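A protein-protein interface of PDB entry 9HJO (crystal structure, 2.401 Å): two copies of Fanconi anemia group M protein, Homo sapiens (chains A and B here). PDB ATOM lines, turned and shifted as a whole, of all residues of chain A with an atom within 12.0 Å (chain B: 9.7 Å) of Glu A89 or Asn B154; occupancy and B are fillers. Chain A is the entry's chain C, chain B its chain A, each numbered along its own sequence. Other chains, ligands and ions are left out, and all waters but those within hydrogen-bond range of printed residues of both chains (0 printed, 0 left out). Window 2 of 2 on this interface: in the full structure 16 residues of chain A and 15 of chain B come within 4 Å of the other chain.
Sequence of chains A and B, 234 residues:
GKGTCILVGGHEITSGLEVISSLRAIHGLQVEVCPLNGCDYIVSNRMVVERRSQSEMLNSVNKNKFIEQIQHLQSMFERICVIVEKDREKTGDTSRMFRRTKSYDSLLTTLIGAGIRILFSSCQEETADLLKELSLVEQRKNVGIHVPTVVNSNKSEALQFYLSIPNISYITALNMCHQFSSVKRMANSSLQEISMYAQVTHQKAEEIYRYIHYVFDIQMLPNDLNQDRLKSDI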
ATOM      1  N   SER A  15     -14.249   1.497  11.075  1.00  0.00           N
ATOM      2  CA  SER A  15     -13.444   0.411  11.639  1.00  0.00           C
ATOM      3  C   SER A  15     -11.953   0.700  11.794  1.00  0.00           C
ATOM      4  O   SER A  15     -11.251  -0.182  12.302  1.00  0.00           O
ATOM      5  CB  SER A  15     -13.567  -0.806  10.789  1.00  0.00           C
ATOM      6  OG  SER A  15     -12.837  -0.659   9.585  1.00  0.00           O
ATOM      7  N   GLY A  16     -11.450   1.868  11.340  1.00  0.00           N
ATOM      8  CA  GLY A  16     -10.011   2.080  11.248  1.00  0.00           C
ATOM      9  C   GLY A  16      -9.524   3.281  12.049  1.00  0.00           C
ATOM     10  O   GLY A  16      -8.428   3.737  11.794  1.00  0.00           O
ATOM     11  N   LEU A  17     -10.248   3.728  13.073  1.00  0.00           N
ATOM     12  CA  LEU A  17      -9.931   4.987  13.755  1.00  0.00           C
ATOM     13  C   LEU A  17      -8.516   5.005  14.323  1.00  0.00           C
ATOM     14  O   LEU A  17      -7.905   6.065  14.317  1.00  0.00           O
ATOM     15  CB  LEU A  17     -10.918   5.362  14.853  1.00  0.00           C
ATOM     16  CG  LEU A  17     -12.363   5.523  14.392  1.00  0.00           C
ATOM     17  CD1 LEU A  17     -13.238   5.540  15.599  1.00  0.00           C
ATOM     18  CD2 LEU A  17     -12.546   6.756  13.542  1.00  0.00           C
ATOM     19  N   GLU A  18      -8.000   3.866  14.793  1.00  0.00           N
ATOM     20  CA  GLU A  18      -6.654   3.833  15.341  1.00  0.00           C
ATOM     21  C   GLU A  18      -5.602   3.804  14.219  1.00  0.00           C
ATOM     22  O   GLU A  18      -4.531   4.392  14.364  1.00  0.00           O
ATOM     23  CB  GLU A  18      -6.536   2.714  16.374  1.00  0.00           C
ATOM     24  CG  GLU A  18      -5.576   3.039  17.519  1.00  0.00           C
ATOM     25  CD  GLU A  18      -4.892   1.830  18.140  1.00  0.00           C
ATOM     26  OE1 GLU A  18      -5.610   0.827  18.388  1.00  0.00           O
ATOM     27  OE2 GLU A  18      -3.651   1.880  18.366  1.00  0.00           O
ATOM     28  N   VAL A  19      -5.896   3.155  13.082  1.00  0.00           N
ATOM     29  CA  VAL A  19      -5.058   3.271  11.900  1.00  0.00           C
ATOM     30  C   VAL A  19      -4.877   4.744  11.531  1.00  0.00           C
ATOM     31  O   VAL A  19      -3.763   5.223  11.418  1.00  0.00           O
ATOM     32  CB  VAL A  19      -5.561   2.488  10.675  1.00  0.00           C
ATOM     33  CG1 VAL A  19      -4.604   2.663   9.507  1.00  0.00           C
ATOM     34  CG2 VAL A  19      -5.762   0.996  10.980  1.00  0.00           C
ATOM     35  N   ARG A  51      -7.365  -2.977   3.260  1.00  0.00           N
ATOM     36  CA  ARG A  51      -7.320  -3.447   4.632  1.00  0.00           C
ATOM     37  C   ARG A  51      -8.492  -4.389   4.833  1.00  0.00           C
ATOM     38  O   ARG A  51      -9.613  -4.010   4.543  1.00  0.00           O
ATOM     39  CB  ARG A  51      -7.506  -2.295   5.640  1.00  0.00           C
ATOM     40  CG  ARG A  51      -7.507  -2.758   7.085  1.00  0.00           C
ATOM     41  CD  ARG A  51      -6.992  -1.820   8.142  1.00  0.00           C
ATOM     42  NE  ARG A  51      -8.025  -1.012   8.768  1.00  0.00           N
ATOM     43  CZ  ARG A  51      -8.926  -1.365   9.643  1.00  0.00           C
ATOM     44  NH1 ARG A  51      -8.638  -2.136  10.652  1.00  0.00           N
ATOM     45  NH2 ARG A  51     -10.108  -0.783   9.574  1.00  0.00           N
ATOM     46  N   SER A  53      -9.956  -7.530   7.661  1.00  0.00           N
ATOM     47  CA  SER A  53      -9.815  -8.371   8.840  1.00  0.00           C
ATOM     48  C   SER A  53      -9.711  -9.848   8.418  1.00  0.00           C
ATOM     49  O   SER A  53     -10.187 -10.214   7.337  1.00  0.00           O
ATOM     50  CB  SER A  53     -10.958  -8.111   9.760  1.00  0.00           C
ATOM     51  OG  SER A  53     -12.124  -8.759   9.266  1.00  0.00           O
ATOM     52  N   GLN A  54      -9.067 -10.684   9.249  1.00  0.00           N
ATOM     53  CA  GLN A  54      -9.052 -12.135   9.077  1.00  0.00           C
ATOM     54  C   GLN A  54     -10.447 -12.664   8.751  1.00  0.00           C
ATOM     55  O   GLN A  54     -10.612 -13.381   7.775  1.00  0.00           O
ATOM     56  CB  GLN A  54      -8.660 -12.864  10.364  1.00  0.00           C
ATOM     57  CG  GLN A  54      -7.169 -13.083  10.559  1.00  0.00           C
ATOM     58  CD  GLN A  54      -6.841 -13.351  12.004  1.00  0.00           C
ATOM     59  OE1 GLN A  54      -7.676 -13.152  12.896  1.00  0.00           O
ATOM     60  NE2 GLN A  54      -5.607 -13.766  12.241  1.00  0.00           N
ATOM     61  N   SER A  55     -11.446 -12.304   9.590  1.00  0.00           N
ATOM     62  CA  SER A  55     -12.839 -12.722   9.427  1.00  0.00           C
ATOM     63  C   SER A  55     -13.362 -12.423   8.030  1.00  0.00           C
ATOM     64  O   SER A  55     -14.010 -13.272   7.428  1.00  0.00           O
ATOM     65  CB  SER A  55     -13.772 -12.060  10.405  1.00  0.00           C
ATOM     66  OG  SER A  55     -13.364 -12.297  11.736  1.00  0.00           O
ATOM     67  N   GLU A  85      -5.567  -7.896   8.669  1.00  0.00           N
ATOM     68  CA  GLU A  85      -5.438  -7.431  10.038  1.00  0.00           C
ATOM     69  C   GLU A  85      -6.211  -8.372  10.951  1.00  0.00           C
ATOM     70  O   GLU A  85      -7.319  -8.770  10.610  1.00  0.00           O
ATOM     71  CB  GLU A  85      -6.040  -6.042  10.173  1.00  0.00           C
ATOM     72  CG  GLU A  85      -5.806  -5.377  11.524  1.00  0.00           C
ATOM     73  CD  GLU A  85      -6.404  -3.992  11.493  1.00  0.00           C
ATOM     74  OE1 GLU A  85      -5.857  -3.156  10.731  1.00  0.00           O
ATOM     75  OE2 GLU A  85      -7.442  -3.768  12.165  1.00  0.00           O
ATOM     76  N   LYS A  86      -5.628  -8.718  12.101  1.00  0.00           N
ATOM     77  CA  LYS A  86      -6.299  -9.576  13.057  1.00  0.00           C
ATOM     78  C   LYS A  86      -7.534  -8.851  13.579  1.00  0.00           C
ATOM     79  O   LYS A  86      -7.484  -7.654  13.832  1.00  0.00           O
ATOM     80  CB  LYS A  86      -5.466  -9.897  14.295  1.00  0.00           C
ATOM     81  CG  LYS A  86      -4.563 -11.108  14.280  1.00  0.00           C
ATOM     82  CD  LYS A  86      -4.446 -11.811  15.637  1.00  0.00           C
ATOM     83  CE  LYS A  86      -4.256 -10.930  16.856  1.00  0.00           C
ATOM     84  NZ  LYS A  86      -3.927 -11.730  18.037  1.00  0.00           N
ATOM     85  N   ASP A  87      -8.620  -9.591  13.784  1.00  0.00           N
ATOM     86  CA  ASP A  87      -9.837  -9.035  14.358  1.00  0.00           C
ATOM     87  C   ASP A  87      -9.546  -8.499  15.762  1.00  0.00           C
ATOM     88  O   ASP A  87      -8.637  -8.980  16.449  1.00  0.00           O
ATOM     89  CB  ASP A  87     -10.976 -10.049  14.388  1.00  0.00           C
ATOM     90  CG  ASP A  87     -11.207 -10.865  13.116  1.00  0.00           C
ATOM     91  OD1 ASP A  87     -11.437 -10.275  12.054  1.00  0.00           O
ATOM     92  OD2 ASP A  87     -11.174 -12.109  13.194  1.00  0.00           O
ATOM     93  N   ARG A  88     -10.335  -7.500  16.181  1.00  0.00           N
ATOM     94  CA  ARG A  88     -10.202  -6.890  17.504  1.00  0.00           C
ATOM     95  C   ARG A  88     -10.710  -7.877  18.558  1.00  0.00           C
ATOM     96  O   ARG A  88     -11.261  -8.921  18.209  1.00  0.00           O
ATOM     97  CB  ARG A  88     -10.852  -5.501  17.604  1.00  0.00           C
ATOM     98  CG  ARG A  88     -12.113  -5.288  16.779  1.00  0.00           C
ATOM     99  CD  ARG A  88     -12.932  -4.065  17.142  1.00  0.00           C
ATOM    100  NE  ARG A  88     -14.246  -4.209  16.501  1.00  0.00           N
ATOM    101  CZ  ARG A  88     -14.491  -4.207  15.190  1.00  0.00           C
ATOM    102  NH1 ARG A  88     -13.588  -3.754  14.325  1.00  0.00           N
ATOM    103  NH2 ARG A  88     -15.664  -4.634  14.750  1.00  0.00           N
ATOM    104  N   GLU A  89     -10.443  -7.569  19.839  1.00  0.00           N
ATOM    105  CA  GLU A  89     -11.001  -8.298  20.968  1.00  0.00           C
ATOM    106  C   GLU A  89     -12.350  -7.657  21.332  1.00  0.00           C
ATOM    107  O   GLU A  89     -13.367  -8.374  21.199  1.00  0.00           O
ATOM    108  CB  GLU A  89     -10.000  -8.322  22.128  1.00  0.00           C
ATOM    109  CG  GLU A  89      -8.771  -9.175  21.819  1.00  0.00           C
ATOM    110  CD  GLU A  89      -7.558  -8.943  22.707  1.00  0.00           C
ATOM    111  OE1 GLU A  89      -6.516  -8.532  22.155  1.00  0.00           O
ATOM    112  OE2 GLU A  89      -7.639  -9.178  23.933  1.00  0.00           O
ATOM    113  N   PHE A  98      -9.974 -17.484  14.960  1.00  0.00           N
ATOM    114  CA  PHE A  98      -9.352 -17.724  13.628  1.00  0.00           C
ATOM    115  C   PHE A  98      -9.104 -19.225  13.480  1.00  0.00           C
ATOM    116  O   PHE A  98      -8.236 -19.782  14.156  1.00  0.00           O
ATOM    117  CB  PHE A  98      -8.094 -16.858  13.467  1.00  0.00           C
ATOM    118  CG  PHE A  98      -7.194 -17.151  12.265  1.00  0.00           C
ATOM    119  CD1 PHE A  98      -7.714 -17.575  11.039  1.00  0.00           C
ATOM    120  CD2 PHE A  98      -5.807 -17.006  12.369  1.00  0.00           C
ATOM    121  CE1 PHE A  98      -6.874 -17.863   9.968  1.00  0.00           C
ATOM    122  CE2 PHE A  98      -4.970 -17.281  11.289  1.00  0.00           C
ATOM    123  CZ  PHE A  98      -5.504 -17.708  10.091  1.00  0.00           C
ATOM    124  N   SER A 121      -1.028  -8.106   9.918  1.00  0.00           N
ATOM    125  CA  SER A 121      -1.011  -7.180  11.030  1.00  0.00           C
ATOM    126  C   SER A 121      -1.852  -7.736  12.190  1.00  0.00           C
ATOM    127  O   SER A 121      -2.960  -8.221  11.995  1.00  0.00           O
ATOM    128  CB  SER A 121      -1.548  -5.867  10.541  1.00  0.00           C
ATOM    129  OG  SER A 121      -1.828  -5.005  11.628  1.00  0.00           O
ATOM    130  N   SER A 122      -1.368  -7.575  13.416  1.00  0.00           N
ATOM    131  CA  SER A 122      -2.069  -8.058  14.595  1.00  0.00           C
ATOM    132  C   SER A 122      -2.917  -6.967  15.266  1.00  0.00           C
ATOM    133  O   SER A 122      -3.731  -7.280  16.122  1.00  0.00           O
ATOM    134  CB  SER A 122      -1.074  -8.696  15.526  1.00  0.00           C
ATOM    135  OG  SER A 122      -0.261  -9.629  14.806  1.00  0.00           O
ATOM    136  N   CYS A 123      -2.786  -5.697  14.865  1.00  0.00           N
ATOM    137  CA  CYS A 123      -3.589  -4.616  15.420  1.00  0.00           C
ATOM    138  C   CYS A 123      -3.568  -3.412  14.472  1.00  0.00           C
ATOM    139  O   CYS A 123      -2.741  -3.348  13.567  1.00  0.00           O
ATOM    140  CB  CYS A 123      -3.063  -4.221  16.793  1.00  0.00           C
ATOM    141  SG  CYS A 123      -1.282  -3.896  16.800  1.00  0.00           S
ATOM    142  N   GLN A 124      -4.435  -2.427  14.738  1.00  0.00           N
ATOM    143  CA  GLN A 124      -4.525  -1.207  13.954  1.00  0.00           C
ATOM    144  C   GLN A 124      -3.221  -0.396  13.970  1.00  0.00           C
ATOM    145  O   GLN A 124      -2.924   0.276  12.985  1.00  0.00           O
ATOM    146  CB  GLN A 124      -5.710  -0.356  14.415  1.00  0.00           C
ATOM    147  CG  GLN A 124      -7.079  -0.957  14.116  1.00  0.00           C
ATOM    148  CD  GLN A 124      -8.227   0.028  14.247  1.00  0.00           C
ATOM    149  OE1 GLN A 124      -8.153   1.191  13.824  1.00  0.00           O
ATOM    150  NE2 GLN A 124      -9.329  -0.425  14.818  1.00  0.00           N
ATOM    151  N   GLU A 125      -2.466  -0.430  15.077  1.00  0.00           N
ATOM    152  CA  GLU A 125      -1.198   0.289  15.200  1.00  0.00           C
ATOM    153  C   GLU A 125      -0.151  -0.265  14.232  1.00  0.00           C
ATOM    154  O   GLU A 125       0.620   0.493  13.648  1.00  0.00           O
ATOM    155  CB  GLU A 125      -0.741   0.237  16.660  1.00  0.00           C
ATOM    156  CG  GLU A 125       0.591   0.923  16.951  1.00  0.00           C
ATOM    157  CD  GLU A 125       0.898   0.971  18.446  1.00  0.00           C
ATOM    158  OE1 GLU A 125       0.835  -0.095  19.108  1.00  0.00           O
ATOM    159  OE2 GLU A 125       1.200   2.072  18.962  1.00  0.00           O
ATOM    160  N   GLU A 126      -0.150  -1.593  14.076  1.00  0.00           N
ATOM    161  CA  GLU A 126       0.760  -2.329  13.208  1.00  0.00           C
ATOM    162  C   GLU A 126       0.356  -2.153  11.745  1.00  0.00           C
ATOM    163  O   GLU A 126       1.213  -2.186  10.875  1.00  0.00           O
ATOM    164  CB  GLU A 126       0.674  -3.769  13.711  1.00  0.00           C
ATOM    165  CG  GLU A 126       1.766  -4.731  13.278  1.00  0.00           C
ATOM    166  CD  GLU A 126       1.771  -5.965  14.182  1.00  0.00           C
ATOM    167  OE1 GLU A 126       1.929  -5.834  15.426  1.00  0.00           O
ATOM    168  OE2 GLU A 126       1.584  -7.077  13.635  1.00  0.00           O
ATOM    169  N   SER B 153     -10.209  -0.187  20.663  1.00  0.00           N
ATOM    170  CA  SER B 153      -9.014  -1.020  20.958  1.00  0.00           C
ATOM    171  C   SER B 153      -9.230  -1.792  22.260  1.00  0.00           C
ATOM    172  O   SER B 153      -8.569  -1.498  23.255  1.00  0.00           O
ATOM    173  CB  SER B 153      -7.753  -0.174  20.991  1.00  0.00           C
ATOM    174  OG  SER B 153      -7.836   0.852  21.972  1.00  0.00           O
ATOM    175  N   ASN B 154     -10.143  -2.784  22.196  1.00  0.00           N
ATOM    176  CA  ASN B 154     -10.596  -3.664  23.273  1.00  0.00           C
ATOM    177  C   ASN B 154     -11.863  -3.141  23.961  1.00  0.00           C
ATOM    178  O   ASN B 154     -12.391  -3.866  24.794  1.00  0.00           O
ATOM    179  CB  ASN B 154      -9.537  -4.072  24.310  1.00  0.00           C
ATOM    180  CG  ASN B 154      -8.483  -5.005  23.753  1.00  0.00           C
ATOM    181  OD1 ASN B 154      -8.312  -6.120  24.263  1.00  0.00           O
ATOM    182  ND2 ASN B 154      -7.755  -4.583  22.728  1.00  0.00           N
ATOM    183  N   LYS B 155     -12.361  -1.938  23.600  1.00  0.00           N
ATOM    184  CA  LYS B 155     -13.497  -1.300  24.260  1.00  0.00           C
ATOM    185  C   LYS B 155     -14.627  -1.032  23.259  1.00  0.00           C
ATOM    186  O   LYS B 155     -15.473  -0.166  23.485  1.00  0.00           O
ATOM    187  CB  LYS B 155     -12.926  -0.037  24.918  1.00  0.00           C
ATOM    188  CG  LYS B 155     -12.147  -0.250  26.218  1.00  0.00           C
ATOM    189  CD  LYS B 155     -12.961   0.037  27.484  1.00  0.00           C
ATOM    190  CE  LYS B 155     -12.168   0.489  28.687  1.00  0.00           C
ATOM    191  NZ  LYS B 155     -12.998   1.280  29.607  1.00  0.00           N
ATOM    192  N   SER B 156     -14.669  -1.812  22.172  1.00  0.00           N
ATOM    193  CA  SER B 156     -15.417  -1.448  20.976  1.00  0.00           C
ATOM    194  C   SER B 156     -16.874  -1.867  21.131  1.00  0.00           C
ATOM    195  O   SER B 156     -17.784  -1.115  20.774  1.00  0.00           O
ATOM    196  CB  SER B 156     -14.794  -2.075  19.749  1.00  0.00           C
ATOM    197  OG  SER B 156     -15.439  -1.624  18.568  1.00  0.00           O
ATOM    198  N   GLU B 157     -17.067  -3.091  21.655  1.00  0.00           N
ATOM    199  CA  GLU B 157     -18.375  -3.595  22.065  1.00  0.00           C
ATOM    200  C   GLU B 157     -19.014  -2.628  23.064  1.00  0.00           C
ATOM    201  O   GLU B 157     -20.197  -2.293  22.910  1.00  0.00           O
ATOM    202  CB  GLU B 157     -18.376  -5.088  22.429  1.00  0.00           C
ATOM    203  CG  GLU B 157     -17.275  -5.600  23.369  1.00  0.00           C
ATOM    204  CD  GLU B 157     -16.948  -7.098  23.295  1.00  0.00           C
ATOM    205  OE1 GLU B 157     -16.814  -7.747  24.364  1.00  0.00           O
ATOM    206  OE2 GLU B 157     -16.810  -7.641  22.178  1.00  0.00           O
ATOM    207  N   ALA B 158     -18.220  -2.125  24.029  1.00  0.00           N
ATOM    208  CA  ALA B 158     -18.742  -1.227  25.055  1.00  0.00           C
ATOM    209  C   ALA B 158     -19.259   0.076  24.462  1.00  0.00           C
ATOM    210  O   ALA B 158     -20.308   0.550  24.891  1.00  0.00           O
ATOM    211  CB  ALA B 158     -17.702  -0.927  26.099  1.00  0.00           C
ATOM    212  N   LEU B 159     -18.518   0.666  23.501  1.00  0.00           N
ATOM    213  CA  LEU B 159     -18.961   1.905  22.875  1.00  0.00           C
ATOM    214  C   LEU B 159     -20.328   1.755  22.210  1.00  0.00           C
ATOM    215  O   LEU B 159     -21.181   2.620  22.404  1.00  0.00           O
ATOM    216  CB  LEU B 159     -17.953   2.400  21.854  1.00  0.00           C
ATOM    217  CG  LEU B 159     -18.286   3.750  21.217  1.00  0.00           C
ATOM    218  CD1 LEU B 159     -18.425   4.816  22.270  1.00  0.00           C
ATOM    219  CD2 LEU B 159     -17.213   4.090  20.226  1.00  0.00           C
ATOM    220  N   CME B 177     -17.245   5.189  27.741  1.00  0.00           N
ATOM    221  CA  CME B 177     -16.289   4.173  27.333  1.00  0.00           C
ATOM    222  CB  CME B 177     -16.265   4.089  25.816  1.00  0.00           C
ATOM    223  SG  CME B 177     -15.326   2.683  25.166  1.00  0.00           S
ATOM    224  SD  CME B 177     -13.615   3.589  24.604  1.00  0.00           S
ATOM    225  CE  CME B 177     -13.200   2.811  23.014  1.00  0.00           C
ATOM    226  CZ  CME B 177     -13.464   3.686  21.828  1.00  0.00           C
ATOM    227  OH  CME B 177     -13.471   2.922  20.625  1.00  0.00           O
ATOM    228  C   CME B 177     -14.904   4.413  27.935  1.00  0.00           C
ATOM    229  O   CME B 177     -14.203   3.471  28.276  1.00  0.00           O
ATOM    230  N   PHE B 180     -15.556   4.726  32.581  1.00  0.00           N
ATOM    231  CA  PHE B 180     -15.937   3.545  33.346  1.00  0.00           C
ATOM    232  C   PHE B 180     -15.028   2.382  32.964  1.00  0.00           C
ATOM    233  O   PHE B 180     -14.931   2.016  31.800  1.00  0.00           O
ATOM    234  CB  PHE B 180     -17.415   3.204  33.148  1.00  0.00           C
ATOM    235  CG  PHE B 180     -18.287   4.357  33.608  1.00  0.00           C
ATOM    236  CD1 PHE B 180     -18.460   4.603  34.960  1.00  0.00           C
ATOM    237  CD2 PHE B 180     -18.921   5.186  32.695  1.00  0.00           C
ATOM    238  CE1 PHE B 180     -19.250   5.655  35.392  1.00  0.00           C
ATOM    239  CE2 PHE B 180     -19.733   6.222  33.123  1.00  0.00           C
ATOM    240  CZ  PHE B 180     -19.868   6.469  34.477  1.00  0.00           C
ATOM    241  N   SER B 181     -14.352   1.806  33.965  1.00  0.00           N
ATOM    242  CA  SER B 181     -13.463   0.671  33.767  1.00  0.00           C
ATOM    243  C   SER B 181     -14.226  -0.502  33.159  1.00  0.00           C
ATOM    244  O   SER B 181     -13.665  -1.219  32.336  1.00  0.00           O
ATOM    245  CB  SER B 181     -12.832   0.295  35.052  1.00  0.00           C
ATOM    246  OG  SER B 181     -13.790   0.482  36.086  1.00  0.00           O
ATOM    247  N   SER B 182     -15.506  -0.665  33.533  1.00  0.00           N
ATOM    248  CA  SER B 182     -16.350  -1.694  32.948  1.00  0.00           C
ATOM    249  C   SER B 182     -17.761  -1.168  32.761  1.00  0.00           C
ATOM    250  O   SER B 182     -18.121  -0.139  33.318  1.00  0.00           O
ATOM    251  CB  SER B 182     -16.356  -2.921  33.812  1.00  0.00           C
ATOM    252  OG  SER B 182     -17.165  -2.665  34.941  1.00  0.00           O
ATOM    253  N   VAL B 183     -18.559  -1.920  32.006  1.00  0.00           N
ATOM    254  CA  VAL B 183     -19.938  -1.541  31.738  1.00  0.00           C
ATOM    255  C   VAL B 183     -20.749  -1.654  33.026  1.00  0.00           C
ATOM    256  O   VAL B 183     -21.594  -0.790  33.278  1.00  0.00           O
ATOM    257  CB  VAL B 183     -20.589  -2.342  30.596  1.00  0.00           C
ATOM    258  CG1 VAL B 183     -22.021  -1.880  30.340  1.00  0.00           C
ATOM    259  CG2 VAL B 183     -19.785  -2.244  29.304  1.00  0.00           C
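No position is printed for both chains.
Of the 4 pairs that touch across the chains among the printed residues, none has its exchanged pair printed and touching as well.
The side-chain amide oxygen of Gln A124 is in hydrogen-bond range of the backbone NH of Glu A18 (2.8 Å).
Among the printed residues, pairs that only touch across the chains: Glu A18 with Ser B153 (3.5 Å), Arg A88 with Ser B156 (3.5 Å) and Glu A89 with Glu B157 (3.7 Å).
Of the 21 printed residues of chain A, 3 touch a printed residue of chain B.
Printed residues of chain A that touch a printed residue of chain B: Glu A18, Arg A88 and Glu A89.
Along chain A the printed residues that touch a printed residue of chain B span positions 18 to 89.
The side-chain amide oxygen (OD1) of Asn B154 sits close to the side-chain carboxylate (OE2) of Glu A89 (3.1 Å).
Of chain B, only Asn B154 and Glu B157 come within 4 Å of Glu A89.
Asn B154 touches just one residue of chain A: Glu A89 (3.1 Å).
Ser B153 touches just one residue of chain A: Glu A18 (3.5 Å).
No residue of chain A comes within 4 Å of Lys B155.
Printed residues of chain B within 4 Å of Arg A88: Ser B156 (3.5 Å).
Printed residues of chain B within 4 Å of Glu A18: Ser B153.
Of the printed residues of chain A, Glu B157 touches Glu A89.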
